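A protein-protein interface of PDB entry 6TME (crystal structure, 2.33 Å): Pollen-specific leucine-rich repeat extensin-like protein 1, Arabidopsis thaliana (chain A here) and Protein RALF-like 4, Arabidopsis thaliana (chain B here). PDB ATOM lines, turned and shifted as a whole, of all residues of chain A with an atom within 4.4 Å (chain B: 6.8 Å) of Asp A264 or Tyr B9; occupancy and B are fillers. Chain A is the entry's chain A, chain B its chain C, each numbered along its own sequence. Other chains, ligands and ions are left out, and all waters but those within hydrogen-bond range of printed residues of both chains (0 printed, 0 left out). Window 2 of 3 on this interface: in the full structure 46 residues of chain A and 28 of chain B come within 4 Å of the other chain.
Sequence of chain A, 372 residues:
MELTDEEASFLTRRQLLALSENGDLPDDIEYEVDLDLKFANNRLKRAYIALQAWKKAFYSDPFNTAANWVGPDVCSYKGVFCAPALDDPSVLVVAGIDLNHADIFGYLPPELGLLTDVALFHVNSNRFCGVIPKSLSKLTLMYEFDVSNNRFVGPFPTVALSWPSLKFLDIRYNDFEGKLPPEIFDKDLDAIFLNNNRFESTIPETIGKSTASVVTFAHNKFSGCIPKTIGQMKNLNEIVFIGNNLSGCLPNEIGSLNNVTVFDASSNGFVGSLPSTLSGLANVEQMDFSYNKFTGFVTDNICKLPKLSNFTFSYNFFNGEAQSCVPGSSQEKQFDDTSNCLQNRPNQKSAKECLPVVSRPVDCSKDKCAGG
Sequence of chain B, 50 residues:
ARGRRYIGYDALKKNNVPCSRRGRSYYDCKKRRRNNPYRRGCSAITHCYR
The side-chain hydroxyl of Tyr B9 lies within hydrogen-bond range of the side-chain carboxylate of Asp A264 (2.8 Å).
Among the printed residues, merely in contact across the chains: Val A262 with Tyr B6 (3.4 Å), Gln A286 with Tyr B6 (3.5 Å), Val A262 with Tyr B9 (3.7 Å), Ile A242 with Leu B12 (3.8 Å), Gln A286 with Tyr B9 (3.97 Å) and Val A240 with Gly B8 (3.99 Å).
O of Val A262 lies within hydrogen-bond range of N of Ile A239, 3.1 Å away. The backbone carbonyl oxygen (O) of Asp A264 is in hydrogen-bond range of the backbone NH (N) of Phe A241. OD1 of Asp A264 is in hydrogen-bond range of OG of Ser A266. N of Asp A264 lies within hydrogen-bond range of O of Ile A239 (3.3 Å). The backbone NH of Phe A263 is in hydrogen-bond range of the backbone carbonyl oxygen of Gln A286 (3.0 Å).
Of the 11 printed residues of chain A, 5 touch a printed residue of chain B. Of the 9 printed residues of chain B, 4 touch a printed residue of chain A. Printed residues of chain B that touch a printed residue of chain A: Tyr B6, Gly B8, Tyr B9 and Leu B12.
Of chain A, only Val A262 (3.7 Å), Asp A264 (2.8 Å) and Gln A286 (3.97 Å) come within 4 Å of Tyr B9. Of the printed residues of chain A, Leu B12 touches Ile A242. Printed residues of chain B within 4 Å of Val A240: Gly B8 (3.99 Å). Of the printed residues of chain A, Tyr B6 touches Val A262 (3.4 Å) and Gln A286 (3.5 Å). Ala B11 touches none of the printed residues of chain A.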
ATOM      1  N   ILE A 239       5.915 -32.412 -22.436  1.00  0.00           N
ATOM      2  CA  ILE A 239       4.635 -33.105 -22.323  1.00  0.00           C
ATOM      3  C   ILE A 239       4.190 -33.047 -20.868  1.00  0.00           C
ATOM      4  O   ILE A 239       4.970 -33.332 -19.956  1.00  0.00           O
ATOM      5  CB  ILE A 239       4.708 -34.558 -22.839  1.00  0.00           C
ATOM      6  CG1 ILE A 239       3.300 -35.157 -22.947  1.00  0.00           C
ATOM      7  CG2 ILE A 239       5.632 -35.450 -21.973  1.00  0.00           C
ATOM      8  CD1 ILE A 239       3.106 -36.011 -24.186  1.00  0.00           C
ATOM      9  N   VAL A 240       2.946 -32.642 -20.644  1.00  0.00           N
ATOM     10  CA  VAL A 240       2.451 -32.354 -19.304  1.00  0.00           C
ATOM     11  C   VAL A 240       1.139 -33.102 -19.094  1.00  0.00           C
ATOM     12  O   VAL A 240       0.171 -32.871 -19.829  1.00  0.00           O
ATOM     13  CB  VAL A 240       2.265 -30.846 -19.092  1.00  0.00           C
ATOM     14  CG1 VAL A 240       1.843 -30.554 -17.662  1.00  0.00           C
ATOM     15  CG2 VAL A 240       3.571 -30.111 -19.436  1.00  0.00           C
ATOM     16  N   PHE A 241       1.123 -34.007 -18.102  1.00  0.00           N
ATOM     17  CA  PHE A 241      -0.025 -34.827 -17.729  1.00  0.00           C
ATOM     18  C   PHE A 241      -0.584 -34.502 -16.346  1.00  0.00           C
ATOM     19  O   PHE A 241      -1.472 -35.223 -15.877  1.00  0.00           O
ATOM     20  CB  PHE A 241       0.337 -36.316 -17.688  1.00  0.00           C
ATOM     21  CG  PHE A 241       0.787 -36.903 -18.978  1.00  0.00           C
ATOM     22  CD1 PHE A 241      -0.135 -37.319 -19.933  1.00  0.00           C
ATOM     23  CD2 PHE A 241       2.135 -37.152 -19.194  1.00  0.00           C
ATOM     24  CE1 PHE A 241       0.291 -37.903 -21.118  1.00  0.00           C
ATOM     25  CE2 PHE A 241       2.569 -37.733 -20.365  1.00  0.00           C
ATOM     26  CZ  PHE A 241       1.651 -38.116 -21.332  1.00  0.00           C
ATOM     27  N   ILE A 242      -0.055 -33.491 -15.659  1.00  0.00           N
ATOM     28  CA  ILE A 242      -0.450 -33.153 -14.293  1.00  0.00           C
ATOM     29  C   ILE A 242      -1.951 -33.318 -14.052  1.00  0.00           C
ATOM     30  O   ILE A 242      -2.777 -32.686 -14.723  1.00  0.00           O
ATOM     31  CB  ILE A 242      -0.037 -31.710 -13.943  1.00  0.00           C
ATOM     32  CG1 ILE A 242       1.425 -31.475 -14.232  1.00  0.00           C
ATOM     33  CG2 ILE A 242      -0.316 -31.406 -12.467  1.00  0.00           C
ATOM     34  CD1 ILE A 242       1.836 -30.047 -13.958  1.00  0.00           C
ATOM     35  N   VAL A 262      10.957 -31.507 -20.572  1.00  0.00           N
ATOM     36  CA  VAL A 262       9.954 -31.375 -19.530  1.00  0.00           C
ATOM     37  C   VAL A 262       9.074 -32.604 -19.634  1.00  0.00           C
ATOM     38  O   VAL A 262       8.347 -32.766 -20.622  1.00  0.00           O
ATOM     39  CB  VAL A 262       9.090 -30.110 -19.666  1.00  0.00           C
ATOM     40  CG1 VAL A 262       7.983 -30.161 -18.609  1.00  0.00           C
ATOM     41  CG2 VAL A 262       9.913 -28.832 -19.532  1.00  0.00           C
ATOM     42  N   PHE A 263       9.116 -33.454 -18.617  1.00  0.00           N
ATOM     43  CA  PHE A 263       8.232 -34.611 -18.540  1.00  0.00           C
ATOM     44  C   PHE A 263       7.574 -34.595 -17.164  1.00  0.00           C
ATOM     45  O   PHE A 263       8.210 -34.914 -16.153  1.00  0.00           O
ATOM     46  CB  PHE A 263       8.986 -35.926 -18.788  1.00  0.00           C
ATOM     47  CG  PHE A 263       8.059 -37.097 -18.989  1.00  0.00           C
ATOM     48  CD1 PHE A 263       7.488 -37.733 -17.904  1.00  0.00           C
ATOM     49  CD2 PHE A 263       7.699 -37.502 -20.259  1.00  0.00           C
ATOM     50  CE1 PHE A 263       6.599 -38.772 -18.087  1.00  0.00           C
ATOM     51  CE2 PHE A 263       6.803 -38.536 -20.447  1.00  0.00           C
ATOM     52  CZ  PHE A 263       6.258 -39.174 -19.366  1.00  0.00           C
ATOM     53  N   ASP A 264       6.301 -34.242 -17.119  1.00  0.00           N
ATOM     54  CA  ASP A 264       5.582 -34.097 -15.857  1.00  0.00           C
ATOM     55  C   ASP A 264       4.381 -35.044 -15.861  1.00  0.00           C
ATOM     56  O   ASP A 264       3.430 -34.851 -16.625  1.00  0.00           O
ATOM     57  CB  ASP A 264       5.172 -32.640 -15.641  1.00  0.00           C
ATOM     58  CG  ASP A 264       4.752 -32.354 -14.198  1.00  0.00           C
ATOM     59  OD1 ASP A 264       4.102 -33.229 -13.576  1.00  0.00           O
ATOM     60  OD2 ASP A 264       5.059 -31.247 -13.693  1.00  0.00           O
ATOM     61  N   ALA A 265       4.436 -36.077 -15.017  1.00  0.00           N
ATOM     62  CA  ALA A 265       3.388 -37.084 -14.907  1.00  0.00           C
ATOM     63  C   ALA A 265       2.713 -37.044 -13.545  1.00  0.00           C
ATOM     64  O   ALA A 265       2.076 -38.026 -13.139  1.00  0.00           O
ATOM     65  CB  ALA A 265       3.948 -38.481 -15.179  1.00  0.00           C
ATOM     66  N   SER A 266       2.785 -35.909 -12.861  1.00  0.00           N
ATOM     67  CA  SER A 266       2.443 -35.893 -11.451  1.00  0.00           C
ATOM     68  C   SER A 266       0.929 -35.875 -11.241  1.00  0.00           C
ATOM     69  O   SER A 266       0.142 -35.500 -12.127  1.00  0.00           O
ATOM     70  CB  SER A 266       3.094 -34.697 -10.745  1.00  0.00           C
ATOM     71  OG  SER A 266       2.554 -33.467 -11.186  1.00  0.00           O
ATOM     72  N   GLN A 286      13.307 -30.835 -16.462  1.00  0.00           N
ATOM     73  CA  GLN A 286      12.273 -30.880 -15.440  1.00  0.00           C
ATOM     74  C   GLN A 286      11.601 -32.234 -15.551  1.00  0.00           C
ATOM     75  O   GLN A 286      11.127 -32.606 -16.629  1.00  0.00           O
ATOM     76  CB  GLN A 286      11.253 -29.750 -15.640  1.00  0.00           C
ATOM     77  CG  GLN A 286      11.849 -28.345 -15.661  1.00  0.00           C
ATOM     78  CD  GLN A 286      12.192 -27.834 -14.269  1.00  0.00           C
ATOM     79  OE1 GLN A 286      11.498 -28.127 -13.282  1.00  0.00           O
ATOM     80  NE2 GLN A 286      13.254 -27.062 -14.184  1.00  0.00           N
ATOM     81  N   ASP A 288       8.926 -34.637 -13.156  1.00  0.00           N
ATOM     82  CA  ASP A 288       8.044 -34.614 -11.990  1.00  0.00           C
ATOM     83  C   ASP A 288       7.186 -35.871 -12.013  1.00  0.00           C
ATOM     84  O   ASP A 288       6.329 -36.021 -12.891  1.00  0.00           O
ATOM     85  CB  ASP A 288       7.147 -33.363 -11.992  1.00  0.00           C
ATOM     86  CG  ASP A 288       6.334 -33.208 -10.685  1.00  0.00           C
ATOM     87  OD1 ASP A 288       6.275 -34.146  -9.870  1.00  0.00           O
ATOM     88  OD2 ASP A 288       5.747 -32.135 -10.461  1.00  0.00           O
ATOM     89  N   ARG B   5      11.996 -20.510 -18.446  1.00  0.00           N
ATOM     90  CA  ARG B   5      10.557 -20.718 -18.455  1.00  0.00           C
ATOM     91  C   ARG B   5      10.203 -21.664 -19.596  1.00  0.00           C
ATOM     92  O   ARG B   5      10.838 -21.655 -20.651  1.00  0.00           O
ATOM     93  CB  ARG B   5       9.798 -19.394 -18.604  1.00  0.00           C
ATOM     94  CG  ARG B   5      10.171 -18.680 -19.884  1.00  0.00           C
ATOM     95  CD  ARG B   5       9.408 -17.390 -20.136  1.00  0.00           C
ATOM     96  NE  ARG B   5       9.682 -16.921 -21.496  1.00  0.00           N
ATOM     97  CZ  ARG B   5       9.018 -15.948 -22.110  1.00  0.00           C
ATOM     98  NH1 ARG B   5       8.036 -15.313 -21.486  1.00  0.00           N
ATOM     99  NH2 ARG B   5       9.342 -15.612 -23.350  1.00  0.00           N
ATOM    100  N   TYR B   6       9.211 -22.503 -19.370  1.00  0.00           N
ATOM    101  CA  TYR B   6       8.807 -23.518 -20.331  1.00  0.00           C
ATOM    102  C   TYR B   6       7.364 -23.249 -20.720  1.00  0.00           C
ATOM    103  O   TYR B   6       6.527 -22.983 -19.851  1.00  0.00           O
ATOM    104  CB  TYR B   6       8.942 -24.922 -19.739  1.00  0.00           C
ATOM    105  CG  TYR B   6      10.324 -25.246 -19.224  1.00  0.00           C
ATOM    106  CD1 TYR B   6      11.290 -25.795 -20.066  1.00  0.00           C
ATOM    107  CD2 TYR B   6      10.663 -25.016 -17.898  1.00  0.00           C
ATOM    108  CE1 TYR B   6      12.555 -26.098 -19.599  1.00  0.00           C
ATOM    109  CE2 TYR B   6      11.932 -25.312 -17.423  1.00  0.00           C
ATOM    110  CZ  TYR B   6      12.874 -25.854 -18.276  1.00  0.00           C
ATOM    111  OH  TYR B   6      14.148 -26.162 -17.809  1.00  0.00           O
ATOM    112  N   ILE B   7       7.070 -23.299 -22.017  1.00  0.00           N
ATOM    113  CA  ILE B   7       5.728 -22.909 -22.409  1.00  0.00           C
ATOM    114  C   ILE B   7       4.718 -23.964 -21.972  1.00  0.00           C
ATOM    115  O   ILE B   7       3.533 -23.655 -21.779  1.00  0.00           O
ATOM    116  CB  ILE B   7       5.673 -22.643 -23.924  1.00  0.00           C
ATOM    117  CG1 ILE B   7       4.288 -22.086 -24.321  1.00  0.00           C
ATOM    118  CG2 ILE B   7       6.018 -23.908 -24.675  1.00  0.00           C
ATOM    119  CD1 ILE B   7       4.214 -21.556 -25.709  1.00  0.00           C
ATOM    120  N   GLY B   8       5.157 -25.220 -21.822  1.00  0.00           N
ATOM    121  CA  GLY B   8       4.260 -26.256 -21.324  1.00  0.00           C
ATOM    122  C   GLY B   8       3.797 -25.978 -19.904  1.00  0.00           C
ATOM    123  O   GLY B   8       2.643 -26.228 -19.553  1.00  0.00           O
ATOM    124  N   TYR B   9       4.689 -25.430 -19.079  1.00  0.00           N
ATOM    125  CA  TYR B   9       4.341 -24.998 -17.734  1.00  0.00           C
ATOM    126  C   TYR B   9       3.595 -23.666 -17.740  1.00  0.00           C
ATOM    127  O   TYR B   9       2.626 -23.491 -16.996  1.00  0.00           O
ATOM    128  CB  TYR B   9       5.605 -24.898 -16.889  1.00  0.00           C
ATOM    129  CG  TYR B   9       6.053 -26.227 -16.350  1.00  0.00           C
ATOM    130  CD1 TYR B   9       5.115 -27.192 -16.004  1.00  0.00           C
ATOM    131  CD2 TYR B   9       7.411 -26.537 -16.210  1.00  0.00           C
ATOM    132  CE1 TYR B   9       5.492 -28.413 -15.509  1.00  0.00           C
ATOM    133  CE2 TYR B   9       7.811 -27.780 -15.713  1.00  0.00           C
ATOM    134  CZ  TYR B   9       6.836 -28.708 -15.355  1.00  0.00           C
ATOM    135  OH  TYR B   9       7.181 -29.944 -14.866  1.00  0.00           O
ATOM    136  N   ASP B  10       4.022 -22.718 -18.571  1.00  0.00           N
ATOM    137  CA  ASP B  10       3.295 -21.451 -18.656  1.00  0.00           C
ATOM    138  C   ASP B  10       1.865 -21.649 -19.113  1.00  0.00           C
ATOM    139  O   ASP B  10       0.988 -20.879 -18.716  1.00  0.00           O
ATOM    140  CB  ASP B  10       4.006 -20.472 -19.580  1.00  0.00           C
ATOM    141  CG  ASP B  10       5.239 -19.871 -18.924  1.00  0.00           C
ATOM    142  OD1 ASP B  10       5.428 -20.126 -17.713  1.00  0.00           O
ATOM    143  OD2 ASP B  10       6.006 -19.146 -19.603  1.00  0.00           O
ATOM    144  N   ALA B  11       1.605 -22.679 -19.927  1.00  0.00           N
ATOM    145  CA  ALA B  11       0.245 -22.998 -20.343  1.00  0.00           C
ATOM    146  C   ALA B  11      -0.682 -23.227 -19.160  1.00  0.00           C
ATOM    147  O   ALA B  11      -1.908 -23.151 -19.325  1.00  0.00           O
ATOM    148  CB  ALA B  11       0.244 -24.237 -21.241  1.00  0.00           C
ATOM    149  N   LEU B  12      -0.122 -23.491 -17.972  1.00  0.00           N
ATOM    150  CA  LEU B  12      -0.902 -23.664 -16.753  1.00  0.00           C
ATOM    151  C   LEU B  12      -1.395 -22.351 -16.167  1.00  0.00           C
ATOM    152  O   LEU B  12      -2.203 -22.384 -15.234  1.00  0.00           O
ATOM    153  CB  LEU B  12      -0.099 -24.411 -15.682  1.00  0.00           C
ATOM    154  CG  LEU B  12       0.091 -25.907 -15.942  1.00  0.00           C
ATOM    155  CD1 LEU B  12       0.833 -26.532 -14.799  1.00  0.00           C
ATOM    156  CD2 LEU B  12      -1.260 -26.569 -16.128  1.00  0.00           C
ATOM    157  N   LYS B  13      -0.950 -21.203 -16.678  1.00  0.00           N
ATOM    158  CA  LYS B  13      -1.485 -19.915 -16.252  1.00  0.00           C
ATOM    159  C   LYS B  13      -2.469 -19.410 -17.305  1.00  0.00           C
ATOM    160  O   LYS B  13      -2.091 -19.165 -18.456  1.00  0.00           O
ATOM    161  CB  LYS B  13      -0.366 -18.908 -15.999  1.00  0.00           C
ATOM    162  CG  LYS B  13       0.662 -19.365 -14.946  1.00  0.00           C
ATOM    163  CD  LYS B  13       1.991 -18.627 -15.152  1.00  0.00           C
ATOM    164  CE  LYS B  13       3.172 -19.355 -14.493  1.00  0.00           C
ATOM    165  NZ  LYS B  13       4.457 -18.599 -14.656  1.00  0.00           N
